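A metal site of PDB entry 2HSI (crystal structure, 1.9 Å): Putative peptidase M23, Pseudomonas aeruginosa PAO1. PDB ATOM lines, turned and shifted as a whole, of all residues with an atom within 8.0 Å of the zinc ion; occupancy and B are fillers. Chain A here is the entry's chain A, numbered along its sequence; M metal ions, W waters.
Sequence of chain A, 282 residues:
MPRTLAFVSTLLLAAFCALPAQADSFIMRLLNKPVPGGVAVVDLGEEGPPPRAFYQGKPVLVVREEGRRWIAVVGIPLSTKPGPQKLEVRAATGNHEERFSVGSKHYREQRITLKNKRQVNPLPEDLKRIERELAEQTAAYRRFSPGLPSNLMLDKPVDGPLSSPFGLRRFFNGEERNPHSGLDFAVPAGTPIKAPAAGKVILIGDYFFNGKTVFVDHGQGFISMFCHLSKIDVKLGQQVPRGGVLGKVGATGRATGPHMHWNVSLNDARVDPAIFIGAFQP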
ATOM      1  N   SER A 163      27.437 -16.722  15.977  1.00  0.00           N
ATOM      2  CA  SER A 163      27.251 -17.832  15.058  1.00  0.00           C
ATOM      3  C   SER A 163      25.843 -18.417  15.234  1.00  0.00           C
ATOM      4  O   SER A 163      24.856 -17.764  14.893  1.00  0.00           O
ATOM      5  CB  SER A 163      28.355 -18.878  15.255  1.00  0.00           C
ATOM      6  OG  SER A 163      28.205 -19.967  14.375  1.00  0.00           O
ATOM      7  N   SER A 164      25.753 -19.627  15.780  1.00  0.00           N
ATOM      8  CA  SER A 164      24.471 -20.279  16.010  1.00  0.00           C
ATOM      9  C   SER A 164      23.652 -19.664  17.168  1.00  0.00           C
ATOM     10  O   SER A 164      24.203 -19.377  18.240  1.00  0.00           O
ATOM     11  CB  SER A 164      24.657 -21.783  16.248  1.00  0.00           C
ATOM     12  OG  SER A 164      25.065 -22.437  15.061  1.00  0.00           O
ATOM     13  N   PRO A 165      22.338 -19.439  16.942  1.00  0.00           N
ATOM     14  CA  PRO A 165      21.251 -19.222  17.913  1.00  0.00           C
ATOM     15  C   PRO A 165      20.998 -20.564  18.664  1.00  0.00           C
ATOM     16  O   PRO A 165      21.410 -21.587  18.107  1.00  0.00           O
ATOM     17  CB  PRO A 165      20.072 -18.865  17.004  1.00  0.00           C
ATOM     18  CG  PRO A 165      20.660 -18.453  15.706  1.00  0.00           C
ATOM     19  CD  PRO A 165      21.831 -19.348  15.556  1.00  0.00           C
ATOM     20  N   PHE A 166      20.340 -20.665  19.835  1.00  0.00           N
ATOM     21  CA  PHE A 166      19.255 -19.845  20.428  1.00  0.00           C
ATOM     22  C   PHE A 166      18.377 -18.917  19.579  1.00  0.00           C
ATOM     23  O   PHE A 166      17.346 -19.323  19.059  1.00  0.00           O
ATOM     24  CB  PHE A 166      19.631 -19.166  21.762  1.00  0.00           C
ATOM     25  CG  PHE A 166      18.773 -19.613  22.925  1.00  0.00           C
ATOM     26  CD1 PHE A 166      19.330 -20.283  23.998  1.00  0.00           C
ATOM     27  CD2 PHE A 166      17.395 -19.386  22.928  1.00  0.00           C
ATOM     28  CE1 PHE A 166      18.543 -20.715  25.076  1.00  0.00           C
ATOM     29  CE2 PHE A 166      16.590 -19.813  23.999  1.00  0.00           C
ATOM     30  CZ  PHE A 166      17.168 -20.482  25.071  1.00  0.00           C
ATOM     31  N   HIS A 180      19.393 -26.216  20.628  1.00  0.00           N
ATOM     32  CA  HIS A 180      20.609 -25.461  20.939  1.00  0.00           C
ATOM     33  C   HIS A 180      20.355 -24.501  22.104  1.00  0.00           C
ATOM     34  O   HIS A 180      19.690 -23.469  21.941  1.00  0.00           O
ATOM     35  CB  HIS A 180      21.115 -24.727  19.697  1.00  0.00           C
ATOM     36  CG  HIS A 180      22.513 -24.196  19.823  1.00  0.00           C
ATOM     37  ND1 HIS A 180      22.825 -22.862  19.690  1.00  0.00           N
ATOM     38  CD2 HIS A 180      23.686 -24.836  20.065  1.00  0.00           C
ATOM     39  CE1 HIS A 180      24.136 -22.703  19.842  1.00  0.00           C
ATOM     40  NE2 HIS A 180      24.674 -23.890  20.075  1.00  0.00           N
ATOM     41  N   SER A 181      20.879 -24.862  23.267  1.00  0.00           N
ATOM     42  CA  SER A 181      20.522 -24.225  24.542  1.00  0.00           C
ATOM     43  C   SER A 181      21.336 -22.971  24.892  1.00  0.00           C
ATOM     44  O   SER A 181      21.183 -22.421  26.001  1.00  0.00           O
ATOM     45  CB  SER A 181      20.593 -25.238  25.686  1.00  0.00           C
ATOM     46  OG  SER A 181      21.890 -25.804  25.781  1.00  0.00           O
ATOM     47  N   GLY A 182      22.165 -22.511  23.959  1.00  0.00           N
ATOM     48  CA  GLY A 182      22.964 -21.295  24.144  1.00  0.00           C
ATOM     49  C   GLY A 182      23.278 -20.537  22.873  1.00  0.00           C
ATOM     50  O   GLY A 182      22.615 -20.724  21.850  1.00  0.00           O
ATOM     51  N   LEU A 183      24.297 -19.679  22.933  1.00  0.00           N
ATOM     52  CA  LEU A 183      24.710 -18.846  21.808  1.00  0.00           C
ATOM     53  C   LEU A 183      26.152 -19.150  21.380  1.00  0.00           C
ATOM     54  O   LEU A 183      27.056 -19.214  22.218  1.00  0.00           O
ATOM     55  CB  LEU A 183      24.562 -17.365  22.177  1.00  0.00           C
ATOM     56  CG  LEU A 183      25.060 -16.252  21.247  1.00  0.00           C
ATOM     57  CD1 LEU A 183      24.317 -16.259  19.907  1.00  0.00           C
ATOM     58  CD2 LEU A 183      24.952 -14.893  21.938  1.00  0.00           C
ATOM     59  N   ASP A 184      26.355 -19.336  20.075  1.00  0.00           N
ATOM     60  CA  ASP A 184      27.701 -19.573  19.542  1.00  0.00           C
ATOM     61  C   ASP A 184      28.341 -18.296  19.005  1.00  0.00           C
ATOM     62  O   ASP A 184      27.642 -17.370  18.586  1.00  0.00           O
ATOM     63  CB  ASP A 184      27.669 -20.615  18.419  1.00  0.00           C
ATOM     64  CG  ASP A 184      27.674 -22.022  18.942  1.00  0.00           C
ATOM     65  OD1 ASP A 184      27.639 -22.217  20.185  1.00  0.00           O
ATOM     66  OD2 ASP A 184      27.707 -22.950  18.114  1.00  0.00           O
ATOM     67  N   PHE A 185      29.674 -18.283  19.018  1.00  0.00           N
ATOM     68  CA  PHE A 185      30.457 -17.223  18.403  1.00  0.00           C
ATOM     69  C   PHE A 185      31.480 -17.850  17.459  1.00  0.00           C
ATOM     70  O   PHE A 185      32.107 -18.863  17.795  1.00  0.00           O
ATOM     71  CB  PHE A 185      31.179 -16.381  19.458  1.00  0.00           C
ATOM     72  CG  PHE A 185      30.258 -15.612  20.364  1.00  0.00           C
ATOM     73  CD1 PHE A 185      29.911 -14.306  20.072  1.00  0.00           C
ATOM     74  CD2 PHE A 185      29.750 -16.196  21.524  1.00  0.00           C
ATOM     75  CE1 PHE A 185      29.057 -13.578  20.917  1.00  0.00           C
ATOM     76  CE2 PHE A 185      28.895 -15.497  22.374  1.00  0.00           C
ATOM     77  CZ  PHE A 185      28.549 -14.178  22.065  1.00  0.00           C
ATOM     78  N   CYS A 227      31.509 -23.904  27.636  1.00  0.00           N
ATOM     79  CA  CYS A 227      32.007 -25.254  27.441  1.00  0.00           C
ATOM     80  C   CYS A 227      32.863 -25.396  26.177  1.00  0.00           C
ATOM     81  O   CYS A 227      32.997 -24.451  25.400  1.00  0.00           O
ATOM     82  CB  CYS A 227      30.860 -26.263  27.480  1.00  0.00           C
ATOM     83  SG  CYS A 227      29.615 -25.996  26.211  1.00  0.00           S
ATOM     84  N   HIS A 228      33.441 -26.591  26.009  1.00  0.00           N
ATOM     85  CA  HIS A 228      34.416 -26.928  24.949  1.00  0.00           C
ATOM     86  C   HIS A 228      35.713 -26.116  25.004  1.00  0.00           C
ATOM     87  O   HIS A 228      36.377 -25.975  23.994  1.00  0.00           O
ATOM     88  CB  HIS A 228      33.801 -26.826  23.533  1.00  0.00           C
ATOM     89  CG  HIS A 228      32.485 -27.527  23.383  1.00  0.00           C
ATOM     90  ND1 HIS A 228      32.359 -28.897  23.463  1.00  0.00           N
ATOM     91  CD2 HIS A 228      31.245 -27.050  23.158  1.00  0.00           C
ATOM     92  CE1 HIS A 228      31.094 -29.237  23.285  1.00  0.00           C
ATOM     93  NE2 HIS A 228      30.392 -28.127  23.102  1.00  0.00           N
ATOM     94  N   HIS A 259      34.511 -24.533  19.032  1.00  0.00           N
ATOM     95  CA  HIS A 259      33.108 -24.294  19.365  1.00  0.00           C
ATOM     96  C   HIS A 259      33.000 -23.468  20.657  1.00  0.00           C
ATOM     97  O   HIS A 259      32.957 -24.006  21.772  1.00  0.00           O
ATOM     98  CB  HIS A 259      32.343 -25.628  19.433  1.00  0.00           C
ATOM     99  CG  HIS A 259      30.892 -25.499  19.778  1.00  0.00           C
ATOM    100  ND1 HIS A 259      30.134 -26.583  20.193  1.00  0.00           N
ATOM    101  CD2 HIS A 259      30.050 -24.440  19.778  1.00  0.00           C
ATOM    102  CE1 HIS A 259      28.904 -26.184  20.432  1.00  0.00           C
ATOM    103  NE2 HIS A 259      28.822 -24.893  20.193  1.00  0.00           N
ATOM    104  N   MET A 260      32.946 -22.159  20.476  1.00  0.00           N
ATOM    105  CA  MET A 260      32.669 -21.206  21.552  1.00  0.00           C
ATOM    106  C   MET A 260      31.170 -21.219  21.885  1.00  0.00           C
ATOM    107  O   MET A 260      30.359 -20.678  21.146  1.00  0.00           O
ATOM    108  CB  MET A 260      33.153 -19.819  21.102  1.00  0.00           C
ATOM    109  CG  MET A 260      32.752 -18.661  21.993  1.00  0.00           C
ATOM    110  SD  MET A 260      33.210 -18.867  23.709  1.00  0.00           S
ATOM    111  CE  MET A 260      32.039 -17.744  24.466  1.00  0.00           C
ATOM    112  N   HIS A 261      30.819 -21.874  22.989  1.00  0.00           N
ATOM    113  CA  HIS A 261      29.419 -21.986  23.419  1.00  0.00           C
ATOM    114  C   HIS A 261      29.205 -21.301  24.762  1.00  0.00           C
ATOM    115  O   HIS A 261      29.919 -21.575  25.730  1.00  0.00           O
ATOM    116  CB  HIS A 261      28.964 -23.451  23.477  1.00  0.00           C
ATOM    117  CG  HIS A 261      27.519 -23.630  23.829  1.00  0.00           C
ATOM    118  ND1 HIS A 261      26.540 -23.819  22.877  1.00  0.00           N
ATOM    119  CD2 HIS A 261      26.883 -23.661  25.025  1.00  0.00           C
ATOM    120  CE1 HIS A 261      25.362 -23.946  23.473  1.00  0.00           C
ATOM    121  NE2 HIS A 261      25.545 -23.848  24.778  1.00  0.00           N
ATOM    122  N   TRP A 262      28.190 -20.436  24.803  1.00  0.00           N
ATOM    123  CA  TRP A 262      27.822 -19.667  26.004  1.00  0.00           C
ATOM    124  C   TRP A 262      26.360 -19.899  26.360  1.00  0.00           C
ATOM    125  O   TRP A 262      25.460 -19.632  25.553  1.00  0.00           O
ATOM    126  CB  TRP A 262      28.092 -18.178  25.752  1.00  0.00           C
ATOM    127  CG  TRP A 262      27.700 -17.200  26.861  1.00  0.00           C
ATOM    128  CD1 TRP A 262      27.688 -17.438  28.210  1.00  0.00           C
ATOM    129  CD2 TRP A 262      27.291 -15.834  26.689  1.00  0.00           C
ATOM    130  NE1 TRP A 262      27.299 -16.302  28.882  1.00  0.00           N
ATOM    131  CE2 TRP A 262      27.051 -15.309  27.978  1.00  0.00           C
ATOM    132  CE3 TRP A 262      27.101 -15.012  25.564  1.00  0.00           C
ATOM    133  CZ2 TRP A 262      26.620 -13.988  28.178  1.00  0.00           C
ATOM    134  CZ3 TRP A 262      26.674 -13.707  25.768  1.00  0.00           C
ATOM    135  CH2 TRP A 262      26.434 -13.203  27.069  1.00  0.00           C
ATOM    136  N   ASN A 263      26.125 -20.433  27.571  1.00  0.00           N
ATOM    137  CA  ASN A 263      24.776 -20.528  28.143  1.00  0.00           C
ATOM    138  C   ASN A 263      24.552 -19.441  29.158  1.00  0.00           C
ATOM    139  O   ASN A 263      25.466 -19.105  29.902  1.00  0.00           O
ATOM    140  CB  ASN A 263      24.582 -21.869  28.861  1.00  0.00           C
ATOM    141  CG  ASN A 263      24.489 -23.042  27.909  1.00  0.00           C
ATOM    142  OD1 ASN A 263      23.941 -22.928  26.822  1.00  0.00           O
ATOM    143  ND2 ASN A 263      25.028 -24.177  28.322  1.00  0.00           N
HETATM  144 ZN    ZN M   1      26.751 -23.878  20.780  1.00  0.00          ZN
HETATM  145  O   HOH W   1      25.852 -26.792  21.251  1.00  0.00           O
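The backbone NH (N) of Phe 166 is in hydrogen-bond range of a ring nitrogen (ND1) of His 180, 3.3 Å away. The side-chain amide oxygen (OD1) of Asn 263 lies within hydrogen-bond range of a ring nitrogen (NE2) of His 261. ND1 of His 259 sits close to NE2 of His 228. The backbone NH (N) of Asp 184 lies within hydrogen-bond range of the backbone carbonyl oxygen (O) of Ser 164, at 2.8 Å. A ring nitrogen (ND1) of His 180 sits at hydrogen-bond distance from the backbone carbonyl oxygen (O) of Pro 165 (2.5 Å). A ring nitrogen (ND1) of His 180 sits at hydrogen-bond distance from the backbone carbonyl oxygen of Gly 182, 3.0 Å away. O of Asp 184 is in hydrogen-bond range of N of Ser 163, 2.7 Å away. O of His 261 is in hydrogen-bond range of N of Cys 227 (3.4 Å).
Four residues have an atom within 4 Å of the zinc ion: His 180, Asp 184, His 259 and His 261.
The zinc ion is bound by the side-chain carboxylate (OD1) of Asp 184. The zinc ion is bound by ND1 of His 261 (2.1 Å). A ring nitrogen (NE2) of His 180 binds the zinc ion. The zinc ion is bound by a ring nitrogen (NE2) of His 259. The zinc ion has four donor atoms within binding distance.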
